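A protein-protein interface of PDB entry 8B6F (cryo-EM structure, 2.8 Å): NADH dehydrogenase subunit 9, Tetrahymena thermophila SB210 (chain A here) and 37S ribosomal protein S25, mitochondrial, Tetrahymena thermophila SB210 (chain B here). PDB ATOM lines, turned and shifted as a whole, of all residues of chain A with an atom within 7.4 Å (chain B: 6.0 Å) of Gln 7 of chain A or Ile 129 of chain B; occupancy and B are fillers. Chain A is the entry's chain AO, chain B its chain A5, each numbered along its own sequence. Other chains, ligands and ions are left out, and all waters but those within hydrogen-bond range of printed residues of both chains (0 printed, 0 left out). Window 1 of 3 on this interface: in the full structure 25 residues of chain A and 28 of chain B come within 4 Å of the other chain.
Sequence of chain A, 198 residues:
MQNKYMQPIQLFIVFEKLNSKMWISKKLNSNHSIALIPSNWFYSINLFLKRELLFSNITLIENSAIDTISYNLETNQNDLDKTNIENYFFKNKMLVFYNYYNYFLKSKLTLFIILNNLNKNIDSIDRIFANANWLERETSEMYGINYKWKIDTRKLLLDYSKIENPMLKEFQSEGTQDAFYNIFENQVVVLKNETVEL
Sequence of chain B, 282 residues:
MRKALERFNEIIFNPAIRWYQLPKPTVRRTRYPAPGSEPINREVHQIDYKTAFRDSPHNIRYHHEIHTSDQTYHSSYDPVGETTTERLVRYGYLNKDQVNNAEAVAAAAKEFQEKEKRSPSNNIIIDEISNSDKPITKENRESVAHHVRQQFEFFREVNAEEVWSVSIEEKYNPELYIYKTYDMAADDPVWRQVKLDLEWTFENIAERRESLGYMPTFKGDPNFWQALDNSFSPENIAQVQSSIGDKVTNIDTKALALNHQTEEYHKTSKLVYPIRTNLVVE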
ATOM      1  N   MET A   1     -32.135   3.152 -24.402  1.00  0.00           N
ATOM      2  CA  MET A   1     -31.368   3.574 -23.195  1.00  0.00           C
ATOM      3  C   MET A   1     -32.277   3.708 -21.981  1.00  0.00           C
ATOM      4  O   MET A   1     -32.010   4.500 -21.081  1.00  0.00           O
ATOM      5  CB  MET A   1     -30.652   4.902 -23.450  1.00  0.00           C
ATOM      6  CG  MET A   1     -29.447   4.796 -24.369  1.00  0.00           C
ATOM      7  SD  MET A   1     -28.607   6.378 -24.558  1.00  0.00           S
ATOM      8  CE  MET A   1     -27.116   5.876 -25.410  1.00  0.00           C
ATOM      9  N   TYR A   5     -28.136   3.748 -15.621  1.00  0.00           N
ATOM     10  CA  TYR A   5     -26.727   3.771 -15.983  1.00  0.00           C
ATOM     11  C   TYR A   5     -26.011   4.852 -15.190  1.00  0.00           C
ATOM     12  O   TYR A   5     -26.583   5.910 -14.909  1.00  0.00           O
ATOM     13  CB  TYR A   5     -26.554   4.023 -17.486  1.00  0.00           C
ATOM     14  CG  TYR A   5     -25.149   4.401 -17.888  1.00  0.00           C
ATOM     15  CD1 TYR A   5     -24.202   3.427 -18.181  1.00  0.00           C
ATOM     16  CD2 TYR A   5     -24.769   5.734 -17.980  1.00  0.00           C
ATOM     17  CE1 TYR A   5     -22.916   3.771 -18.551  1.00  0.00           C
ATOM     18  CE2 TYR A   5     -23.487   6.087 -18.349  1.00  0.00           C
ATOM     19  CZ  TYR A   5     -22.566   5.103 -18.633  1.00  0.00           C
ATOM     20  OH  TYR A   5     -21.288   5.454 -19.000  1.00  0.00           O
ATOM     21  N   MET A   6     -24.760   4.578 -14.827  1.00  0.00           N
ATOM     22  CA  MET A   6     -23.916   5.547 -14.145  1.00  0.00           C
ATOM     23  C   MET A   6     -22.517   5.490 -14.738  1.00  0.00           C
ATOM     24  O   MET A   6     -21.999   4.406 -15.020  1.00  0.00           O
ATOM     25  CB  MET A   6     -23.853   5.279 -12.637  1.00  0.00           C
ATOM     26  CG  MET A   6     -23.030   6.305 -11.875  1.00  0.00           C
ATOM     27  SD  MET A   6     -23.002   6.002 -10.102  1.00  0.00           S
ATOM     28  CE  MET A   6     -21.941   7.336  -9.554  1.00  0.00           C
ATOM     29  N   GLN A   7     -21.913   6.658 -14.921  1.00  0.00           N
ATOM     30  CA  GLN A   7     -20.576   6.720 -15.485  1.00  0.00           C
ATOM     31  C   GLN A   7     -19.564   6.118 -14.511  1.00  0.00           C
ATOM     32  O   GLN A   7     -19.711   6.243 -13.294  1.00  0.00           O
ATOM     33  CB  GLN A   7     -20.187   8.162 -15.792  1.00  0.00           C
ATOM     34  CG  GLN A   7     -21.153   8.892 -16.701  1.00  0.00           C
ATOM     35  CD  GLN A   7     -20.755  10.336 -16.911  1.00  0.00           C
ATOM     36  OE1 GLN A   7     -19.601  10.705 -16.711  1.00  0.00           O
ATOM     37  NE2 GLN A   7     -21.714  11.164 -17.305  1.00  0.00           N
ATOM     38  N   PRO A   8     -18.520   5.460 -15.023  1.00  0.00           N
ATOM     39  CA  PRO A   8     -17.442   4.965 -14.147  1.00  0.00           C
ATOM     40  C   PRO A   8     -16.463   6.069 -13.759  1.00  0.00           C
ATOM     41  O   PRO A   8     -15.274   6.032 -14.081  1.00  0.00           O
ATOM     42  CB  PRO A   8     -16.796   3.876 -15.011  1.00  0.00           C
ATOM     43  CG  PRO A   8     -16.976   4.365 -16.399  1.00  0.00           C
ATOM     44  CD  PRO A   8     -18.301   5.075 -16.429  1.00  0.00           C
ATOM     45  N   ILE A   9     -16.979   7.081 -13.052  1.00  0.00           N
ATOM     46  CA  ILE A   9     -16.168   8.232 -12.658  1.00  0.00           C
ATOM     47  C   ILE A   9     -15.277   7.935 -11.464  1.00  0.00           C
ATOM     48  O   ILE A   9     -14.493   8.800 -11.058  1.00  0.00           O
ATOM     49  CB  ILE A   9     -17.096   9.432 -12.374  1.00  0.00           C
ATOM     50  CG1 ILE A   9     -16.318  10.754 -12.370  1.00  0.00           C
ATOM     51  CG2 ILE A   9     -17.830   9.251 -11.054  1.00  0.00           C
ATOM     52  CD1 ILE A   9     -15.729  11.137 -13.713  1.00  0.00           C
ATOM     53  N   GLN A  10     -15.364   6.732 -10.893  1.00  0.00           N
ATOM     54  CA  GLN A  10     -14.517   6.393  -9.755  1.00  0.00           C
ATOM     55  C   GLN A  10     -13.045   6.425 -10.139  1.00  0.00           C
ATOM     56  O   GLN A  10     -12.203   6.903  -9.370  1.00  0.00           O
ATOM     57  CB  GLN A  10     -14.886   5.014  -9.209  1.00  0.00           C
ATOM     58  CG  GLN A  10     -16.268   4.925  -8.594  1.00  0.00           C
ATOM     59  CD  GLN A  10     -17.376   4.922  -9.626  1.00  0.00           C
ATOM     60  OE1 GLN A  10     -17.139   4.672 -10.804  1.00  0.00           O
ATOM     61  NE2 GLN A  10     -18.594   5.209  -9.185  1.00  0.00           N
ATOM     62  N   LEU A  11     -12.714   5.919 -11.328  1.00  0.00           N
ATOM     63  CA  LEU A  11     -11.324   5.896 -11.765  1.00  0.00           C
ATOM     64  C   LEU A  11     -10.722   7.291 -11.757  1.00  0.00           C
ATOM     65  O   LEU A  11      -9.621   7.505 -11.240  1.00  0.00           O
ATOM     66  CB  LEU A  11     -11.223   5.287 -13.163  1.00  0.00           C
ATOM     67  CG  LEU A  11     -11.360   3.770 -13.270  1.00  0.00           C
ATOM     68  CD1 LEU A  11     -11.373   3.347 -14.730  1.00  0.00           C
ATOM     69  CD2 LEU A  11     -10.240   3.084 -12.508  1.00  0.00           C
ATOM     70  N   PHE A  12     -11.433   8.258 -12.327  1.00  0.00           N
ATOM     71  CA  PHE A  12     -10.909   9.610 -12.431  1.00  0.00           C
ATOM     72  C   PHE A  12     -11.039  10.389 -11.128  1.00  0.00           C
ATOM     73  O   PHE A  12     -10.318  11.375 -10.941  1.00  0.00           O
ATOM     74  CB  PHE A  12     -11.618  10.342 -13.569  1.00  0.00           C
ATOM     75  CG  PHE A  12     -11.629   9.568 -14.855  1.00  0.00           C
ATOM     76  CD1 PHE A  12     -10.541   9.607 -15.710  1.00  0.00           C
ATOM     77  CD2 PHE A  12     -12.721   8.792 -15.202  1.00  0.00           C
ATOM     78  CE1 PHE A  12     -10.544   8.891 -16.890  1.00  0.00           C
ATOM     79  CE2 PHE A  12     -12.732   8.073 -16.382  1.00  0.00           C
ATOM     80  CZ  PHE A  12     -11.641   8.124 -17.227  1.00  0.00           C
ATOM     81  N   SER A  20     -10.750  13.299 -17.915  1.00  0.00           N
ATOM     82  CA  SER A  20     -11.736  12.299 -18.300  1.00  0.00           C
ATOM     83  C   SER A  20     -12.233  12.569 -19.713  1.00  0.00           C
ATOM     84  O   SER A  20     -12.554  13.711 -20.057  1.00  0.00           O
ATOM     85  CB  SER A  20     -12.914  12.300 -17.326  1.00  0.00           C
ATOM     86  OG  SER A  20     -12.469  12.179 -15.989  1.00  0.00           O
ATOM     87  N   LYS A  21     -12.288  11.517 -20.526  1.00  0.00           N
ATOM     88  CA  LYS A  21     -12.868  11.576 -21.869  1.00  0.00           C
ATOM     89  C   LYS A  21     -13.661  10.286 -22.049  1.00  0.00           C
ATOM     90  O   LYS A  21     -13.082   9.231 -22.319  1.00  0.00           O
ATOM     91  CB  LYS A  21     -11.795  11.727 -22.938  1.00  0.00           C
ATOM     92  CG  LYS A  21     -11.052  13.053 -22.902  1.00  0.00           C
ATOM     93  CD  LYS A  21     -11.928  14.190 -23.393  1.00  0.00           C
ATOM     94  CE  LYS A  21     -11.164  15.503 -23.422  1.00  0.00           C
ATOM     95  NZ  LYS A  21     -10.691  15.911 -22.070  1.00  0.00           N
ATOM     96  N   MET A  22     -14.983  10.376 -21.907  1.00  0.00           N
ATOM     97  CA  MET A  22     -15.850   9.209 -21.879  1.00  0.00           C
ATOM     98  C   MET A  22     -16.952   9.338 -22.921  1.00  0.00           C
ATOM     99  O   MET A  22     -17.374  10.441 -23.272  1.00  0.00           O
ATOM    100  CB  MET A  22     -16.472   9.017 -20.491  1.00  0.00           C
ATOM    101  CG  MET A  22     -15.453   8.686 -19.411  1.00  0.00           C
ATOM    102  SD  MET A  22     -16.181   8.495 -17.774  1.00  0.00           S
ATOM    103  CE  MET A  22     -16.720  10.170 -17.444  1.00  0.00           C
ATOM    104  N   TRP A  23     -17.413   8.186 -23.407  1.00  0.00           N
ATOM    105  CA  TRP A  23     -18.444   8.116 -24.430  1.00  0.00           C
ATOM    106  C   TRP A  23     -19.411   6.984 -24.113  1.00  0.00           C
ATOM    107  O   TRP A  23     -19.046   5.989 -23.484  1.00  0.00           O
ATOM    108  CB  TRP A  23     -17.855   7.873 -25.827  1.00  0.00           C
ATOM    109  CG  TRP A  23     -17.075   9.012 -26.397  1.00  0.00           C
ATOM    110  CD1 TRP A  23     -17.553  10.018 -27.179  1.00  0.00           C
ATOM    111  CD2 TRP A  23     -15.671   9.251 -26.246  1.00  0.00           C
ATOM    112  NE1 TRP A  23     -16.538  10.876 -27.520  1.00  0.00           N
ATOM    113  CE2 TRP A  23     -15.371  10.427 -26.959  1.00  0.00           C
ATOM    114  CE3 TRP A  23     -14.640   8.588 -25.572  1.00  0.00           C
ATOM    115  CZ2 TRP A  23     -14.085  10.954 -27.020  1.00  0.00           C
ATOM    116  CZ3 TRP A  23     -13.362   9.113 -25.634  1.00  0.00           C
ATOM    117  CH2 TRP A  23     -13.096  10.286 -26.352  1.00  0.00           C
ATOM    118  N   ILE A  24     -20.654   7.157 -24.553  1.00  0.00           N
ATOM    119  CA  ILE A  24     -21.631   6.077 -24.636  1.00  0.00           C
ATOM    120  C   ILE A  24     -22.434   6.288 -25.909  1.00  0.00           C
ATOM    121  O   ILE A  24     -22.761   7.425 -26.265  1.00  0.00           O
ATOM    122  CB  ILE A  24     -22.565   6.014 -23.409  1.00  0.00           C
ATOM    123  CG1 ILE A  24     -23.447   7.263 -23.333  1.00  0.00           C
ATOM    124  CG2 ILE A  24     -21.743   5.853 -22.139  1.00  0.00           C
ATOM    125  CD1 ILE A  24     -24.444   7.237 -22.199  1.00  0.00           C
ATOM    126  N   SER A  25     -22.748   5.197 -26.598  1.00  0.00           N
ATOM    127  CA  SER A  25     -23.469   5.278 -27.857  1.00  0.00           C
ATOM    128  C   SER A  25     -24.507   4.169 -27.927  1.00  0.00           C
ATOM    129  O   SER A  25     -24.362   3.120 -27.297  1.00  0.00           O
ATOM    130  CB  SER A  25     -22.514   5.176 -29.052  1.00  0.00           C
ATOM    131  OG  SER A  25     -23.216   5.286 -30.277  1.00  0.00           O
ATOM    132  N   SER A  33     -19.626   1.643 -21.722  1.00  0.00           N
ATOM    133  CA  SER A  33     -19.021   2.965 -21.670  1.00  0.00           C
ATOM    134  C   SER A  33     -17.567   2.896 -22.108  1.00  0.00           C
ATOM    135  O   SER A  33     -16.824   2.005 -21.689  1.00  0.00           O
ATOM    136  CB  SER A  33     -19.105   3.551 -20.259  1.00  0.00           C
ATOM    137  OG  SER A  33     -18.525   4.843 -20.211  1.00  0.00           O
ATOM    138  N   ILE A  34     -17.168   3.847 -22.953  1.00  0.00           N
ATOM    139  CA  ILE A  34     -15.801   3.959 -23.447  1.00  0.00           C
ATOM    140  C   ILE A  34     -15.112   5.107 -22.725  1.00  0.00           C
ATOM    141  O   ILE A  34     -15.742   6.101 -22.354  1.00  0.00           O
ATOM    142  CB  ILE A  34     -15.772   4.168 -24.980  1.00  0.00           C
ATOM    143  CG1 ILE A  34     -15.944   2.845 -25.732  1.00  0.00           C
ATOM    144  CG2 ILE A  34     -14.480   4.831 -25.424  1.00  0.00           C
ATOM    145  CD1 ILE A  34     -17.212   2.107 -25.424  1.00  0.00           C
ATOM    146  N   PHE A  55     -15.434  -2.621  -8.437  1.00  0.00           N
ATOM    147  CA  PHE A  55     -14.728  -3.112  -9.611  1.00  0.00           C
ATOM    148  C   PHE A  55     -13.999  -4.421  -9.352  1.00  0.00           C
ATOM    149  O   PHE A  55     -13.319  -4.921 -10.252  1.00  0.00           O
ATOM    150  CB  PHE A  55     -13.729  -2.068 -10.114  1.00  0.00           C
ATOM    151  CG  PHE A  55     -14.369  -0.866 -10.740  1.00  0.00           C
ATOM    152  CD1 PHE A  55     -15.013  -0.968 -11.962  1.00  0.00           C
ATOM    153  CD2 PHE A  55     -14.311   0.368 -10.119  1.00  0.00           C
ATOM    154  CE1 PHE A  55     -15.598   0.135 -12.547  1.00  0.00           C
ATOM    155  CE2 PHE A  55     -14.895   1.476 -10.699  1.00  0.00           C
ATOM    156  CZ  PHE A  55     -15.539   1.360 -11.916  1.00  0.00           C
ATOM    157  N   LEU A 105     -21.796  -3.952 -11.022  1.00  0.00           N
ATOM    158  CA  LEU A 105     -22.464  -2.842 -11.685  1.00  0.00           C
ATOM    159  C   LEU A 105     -23.144  -3.246 -12.985  1.00  0.00           C
ATOM    160  O   LEU A 105     -23.769  -2.395 -13.625  1.00  0.00           O
ATOM    161  CB  LEU A 105     -21.455  -1.725 -11.965  1.00  0.00           C
ATOM    162  CG  LEU A 105     -20.658  -1.238 -10.754  1.00  0.00           C
ATOM    163  CD1 LEU A 105     -19.653  -0.179 -11.165  1.00  0.00           C
ATOM    164  CD2 LEU A 105     -21.583  -0.707  -9.677  1.00  0.00           C
ATOM    165  N   TYR B  73     -23.023  10.170 -26.946  1.00  0.00           N
ATOM    166  CA  TYR B  73     -22.937  11.270 -25.998  1.00  0.00           C
ATOM    167  C   TYR B  73     -21.551  11.283 -25.369  1.00  0.00           C
ATOM    168  O   TYR B  73     -20.988  10.227 -25.069  1.00  0.00           O
ATOM    169  CB  TYR B  73     -24.009  11.140 -24.915  1.00  0.00           C
ATOM    170  CG  TYR B  73     -25.399  10.952 -25.474  1.00  0.00           C
ATOM    171  CD1 TYR B  73     -26.147  12.040 -25.903  1.00  0.00           C
ATOM    172  CD2 TYR B  73     -25.958   9.687 -25.581  1.00  0.00           C
ATOM    173  CE1 TYR B  73     -27.416  11.872 -26.418  1.00  0.00           C
ATOM    174  CE2 TYR B  73     -27.227   9.508 -26.094  1.00  0.00           C
ATOM    175  CZ  TYR B  73     -27.951  10.604 -26.511  1.00  0.00           C
ATOM    176  OH  TYR B  73     -29.215  10.434 -27.024  1.00  0.00           O
ATOM    177  N   HIS B  74     -21.014  12.482 -25.162  1.00  0.00           N
ATOM    178  CA  HIS B  74     -19.653  12.671 -24.684  1.00  0.00           C
ATOM    179  C   HIS B  74     -19.672  13.368 -23.330  1.00  0.00           C
ATOM    180  O   HIS B  74     -20.465  14.285 -23.105  1.00  0.00           O
ATOM    181  CB  HIS B  74     -18.830  13.487 -25.682  1.00  0.00           C
ATOM    182  CG  HIS B  74     -17.386  13.615 -25.309  1.00  0.00           C
ATOM    183  ND1 HIS B  74     -16.643  12.556 -24.836  1.00  0.00           N
ATOM    184  CD2 HIS B  74     -16.546  14.676 -25.351  1.00  0.00           C
ATOM    185  CE1 HIS B  74     -15.409  12.960 -24.595  1.00  0.00           C
ATOM    186  NE2 HIS B  74     -15.323  14.242 -24.900  1.00  0.00           N
ATOM    187  N   SER B  75     -18.795  12.923 -22.435  1.00  0.00           N
ATOM    188  CA  SER B  75     -18.622  13.523 -21.115  1.00  0.00           C
ATOM    189  C   SER B  75     -17.133  13.736 -20.886  1.00  0.00           C
ATOM    190  O   SER B  75     -16.372  12.767 -20.803  1.00  0.00           O
ATOM    191  CB  SER B  75     -19.226  12.643 -20.023  1.00  0.00           C
ATOM    192  OG  SER B  75     -19.352  13.356 -18.806  1.00  0.00           O
ATOM    193  N   TYR B  77     -14.297  15.888 -18.440  1.00  0.00           N
ATOM    194  CA  TYR B  77     -14.039  16.631 -17.217  1.00  0.00           C
ATOM    195  C   TYR B  77     -12.559  16.972 -17.119  1.00  0.00           C
ATOM    196  O   TYR B  77     -11.707  16.269 -17.666  1.00  0.00           O
ATOM    197  CB  TYR B  77     -14.439  15.832 -15.967  1.00  0.00           C
ATOM    198  CG  TYR B  77     -15.820  15.218 -16.003  1.00  0.00           C
ATOM    199  CD1 TYR B  77     -16.046  14.009 -16.646  1.00  0.00           C
ATOM    200  CD2 TYR B  77     -16.889  15.831 -15.368  1.00  0.00           C
ATOM    201  CE1 TYR B  77     -17.301  13.438 -16.671  1.00  0.00           C
ATOM    202  CE2 TYR B  77     -18.147  15.267 -15.387  1.00  0.00           C
ATOM    203  CZ  TYR B  77     -18.347  14.071 -16.037  1.00  0.00           C
ATOM    204  OH  TYR B  77     -19.600  13.506 -16.059  1.00  0.00           O
ATOM    205  N   ASP B 127     -21.067  17.325 -20.253  1.00  0.00           N
ATOM    206  CA  ASP B 127     -21.657  16.137 -19.642  1.00  0.00           C
ATOM    207  C   ASP B 127     -22.874  15.662 -20.429  1.00  0.00           C
ATOM    208  O   ASP B 127     -23.943  15.420 -19.869  1.00  0.00           O
ATOM    209  CB  ASP B 127     -22.032  16.411 -18.189  1.00  0.00           C
ATOM    210  CG  ASP B 127     -22.371  15.149 -17.430  1.00  0.00           C
ATOM    211  OD1 ASP B 127     -22.252  14.054 -18.016  1.00  0.00           O
ATOM    212  OD2 ASP B 127     -22.753  15.247 -16.247  1.00  0.00           O
ATOM    213  N   GLU B 128     -22.735  15.532 -21.749  1.00  0.00           N
ATOM    214  CA  GLU B 128     -23.869  15.085 -22.549  1.00  0.00           C
ATOM    215  C   GLU B 128     -24.408  13.740 -22.080  1.00  0.00           C
ATOM    216  O   GLU B 128     -25.583  13.438 -22.317  1.00  0.00           O
ATOM    217  CB  GLU B 128     -23.481  14.984 -24.025  1.00  0.00           C
ATOM    218  CG  GLU B 128     -23.067  16.296 -24.659  1.00  0.00           C
ATOM    219  CD  GLU B 128     -22.600  16.123 -26.093  1.00  0.00           C
ATOM    220  OE1 GLU B 128     -22.569  14.970 -26.571  1.00  0.00           O
ATOM    221  OE2 GLU B 128     -22.267  17.135 -26.743  1.00  0.00           O
ATOM    222  N   ILE B 129     -23.579  12.922 -21.427  1.00  0.00           N
ATOM    223  CA  ILE B 129     -24.024  11.595 -21.006  1.00  0.00           C
ATOM    224  C   ILE B 129     -25.167  11.703 -20.006  1.00  0.00           C
ATOM    225  O   ILE B 129     -26.203  11.044 -20.147  1.00  0.00           O
ATOM    226  CB  ILE B 129     -22.846  10.785 -20.431  1.00  0.00           C
ATOM    227  CG1 ILE B 129     -21.846  10.447 -21.542  1.00  0.00           C
ATOM    228  CG2 ILE B 129     -23.345   9.539 -19.708  1.00  0.00           C
ATOM    229  CD1 ILE B 129     -20.614   9.688 -21.075  1.00  0.00           C
ATOM    230  N   SER B 130     -24.995  12.534 -18.977  1.00  0.00           N
ATOM    231  CA  SER B 130     -25.976  12.653 -17.908  1.00  0.00           C
ATOM    232  C   SER B 130     -26.344  14.086 -17.555  1.00  0.00           C
ATOM    233  O   SER B 130     -27.305  14.282 -16.802  1.00  0.00           O
ATOM    234  CB  SER B 130     -25.474  11.946 -16.640  1.00  0.00           C
ATOM    235  OG  SER B 130     -24.270  12.529 -16.173  1.00  0.00           O
ATOM    236  N   ASN B 131     -25.626  15.087 -18.063  1.00  0.00           N
ATOM    237  CA  ASN B 131     -25.942  16.488 -17.787  1.00  0.00           C
ATOM    238  C   ASN B 131     -25.981  16.762 -16.287  1.00  0.00           C
ATOM    239  O   ASN B 131     -26.853  17.473 -15.788  1.00  0.00           O
ATOM    240  CB  ASN B 131     -27.267  16.887 -18.440  1.00  0.00           C
ATOM    241  CG  ASN B 131     -27.256  16.691 -19.943  1.00  0.00           C
ATOM    242  OD1 ASN B 131     -27.959  15.830 -20.471  1.00  0.00           O
ATOM    243  ND2 ASN B 131     -26.462  17.496 -20.640  1.00  0.00           N
ATOM    244  N   HIS B 147     -21.153  11.586  -4.191  1.00  0.00           N
ATOM    245  CA  HIS B 147     -20.888  10.618  -5.247  1.00  0.00           C
ATOM    246  C   HIS B 147     -20.929   9.192  -4.712  1.00  0.00           C
ATOM    247  O   HIS B 147     -21.414   8.281  -5.393  1.00  0.00           O
ATOM    248  CB  HIS B 147     -19.535  10.902  -5.895  1.00  0.00           C
ATOM    249  CG  HIS B 147     -19.015   9.761  -6.708  1.00  0.00           C
ATOM    250  ND1 HIS B 147     -18.103   8.853  -6.214  1.00  0.00           N
ATOM    251  CD2 HIS B 147     -19.293   9.364  -7.971  1.00  0.00           C
ATOM    252  CE1 HIS B 147     -17.836   7.952  -7.141  1.00  0.00           C
ATOM    253  NE2 HIS B 147     -18.547   8.238  -8.218  1.00  0.00           N
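A ring nitrogen (ND1) of His 74 of chain B is in hydrogen-bond range of the indole nitrogen (NE1) of Trp 23 of chain A.
A ring nitrogen (NE2) of His 147 of chain B sits at hydrogen-bond distance from the side-chain amide nitrogen of Gln 10 of chain A (3.2 Å).
The side-chain hydroxyl (OG) of Ser 130 of chain B lies within hydrogen-bond range of the side-chain amide nitrogen (NE2) of Gln 7 of chain A (3.1 Å).
The side-chain hydroxyl (OH) of Tyr 77 of chain B sits at hydrogen-bond distance from the side-chain amide oxygen (OE1) of Gln 7 of chain A (2.9 Å).
The backbone NH (N) of Ser 20 of chain A is in hydrogen-bond range of the backbone carbonyl oxygen (O) of Tyr 77 of chain B, at 3.1 Å.
NE2 of Gln 7 of chain A is in hydrogen-bond range of OD1 of Asp 127 of chain B (3.0 Å).
The backbone NH of Tyr 73 of chain B lies within hydrogen-bond range of the backbone carbonyl oxygen of Ile 24 of chain A, at 2.8 Å.
OE1 of Gln 7 of chain A lies within hydrogen-bond range of OG of Ser 75 of chain B (3.4 Å).
O of Ser 75 of chain B lies within hydrogen-bond range of N of Met 22 of chain A (3.0 Å).
O of Met 22 of chain A sits at hydrogen-bond distance from ND1 of His 74 of chain B.
The side-chain hydroxyl (OG) of Ser 75 of chain B sits at hydrogen-bond distance from the side-chain hydroxyl (OH) of Tyr 77 of chain B (2.8 Å).
O of Asp 127 of chain B lies close to ND2 of Asn 131 of chain B, at 3.4 Å.
The side-chain hydroxyl (OG) of Ser 130 of chain B lies within hydrogen-bond range of the side-chain carboxylate (OD2) of Asp 127 of chain B.
The side-chain carboxylate (OD1) of Asp 127 of chain B sits at hydrogen-bond distance from the side-chain hydroxyl (OG) of Ser 75 of chain B, 3.1 Å away.
O of His 74 of chain B is in hydrogen-bond range of N of Glu 128 of chain B, 2.9 Å away.
The backbone NH (N) of Trp 23 of chain A lies within hydrogen-bond range of the backbone carbonyl oxygen (O) of Ile 34 of chain A (2.9 Å).
CE of Met 1 of chain A touches CE2 of Tyr 73 of chain B, 3.7 Å away.
Tyr 5 of chain A touches Ile 129 of chain B.
His 147 of chain B touches Met 6 of chain A (CD2 to CE, 3.7 Å).
Ile 129 of chain B touches Gln 7 of chain A (CG2 to NE2, 3.3 Å).
His 147 of chain B touches Ile 9 of chain A.
Lys 21 of chain A touches His 74 of chain B (CD to NE2, 3.7 Å).
Lys 21 of chain A touches Ser 75 of chain B.
CE1 of Tyr 77 of chain B touches CE of Met 22 of chain A (3.4 Å).
Ile 129 of chain B touches Met 22 of chain A.
Trp 23 of chain A touches Tyr 73 of chain B (CA to O, 3.4 Å).
Gln 7 of chain A touches just these residues of chain B: Ser 75 (3.4 Å), Tyr 77 (2.9 Å), Asp 127 (3.0 Å), Ile 129 (3.3 Å) and Ser 130 (3.1 Å).
Printed residues of chain A within 4 Å of Ile 129 of chain B: Tyr 5 (3.7 Å), Gln 7 (3.3 Å), Met 22 (3.99 Å) and Ile 24 (3.6 Å).
Of the printed residues of chain B, Ile 24 of chain A touches Tyr 73 and Ile 129.
Of the printed residues of chain B, Met 22 of chain A touches His 74, Ser 75, Tyr 77 and Ile 129.
Leu 11 of chain A touches none of the printed residues of chain B.
Phe 55 of chain A touches none of the printed residues of chain B.
The nearest printed residue of chain A that does not touch Ile 129 of chain B is Trp 23 of chain A (4.2 Å).
The nearest printed residue of chain B that does not touch Met 1 of chain A is Ile 129 of chain B (6.9 Å).
Of the 10 printed residues of chain B, 8 touch a printed residue of chain A.
Hydrophobic or aromatic side chains of chain B that line the printed part of chain A: Tyr 73, His 74, Tyr 77, Ile 129 and His 147.
Among the printed residues, no Asp or Glu carboxylate lies within 4 Å of a Lys or Arg side-chain nitrogen of the other chain.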
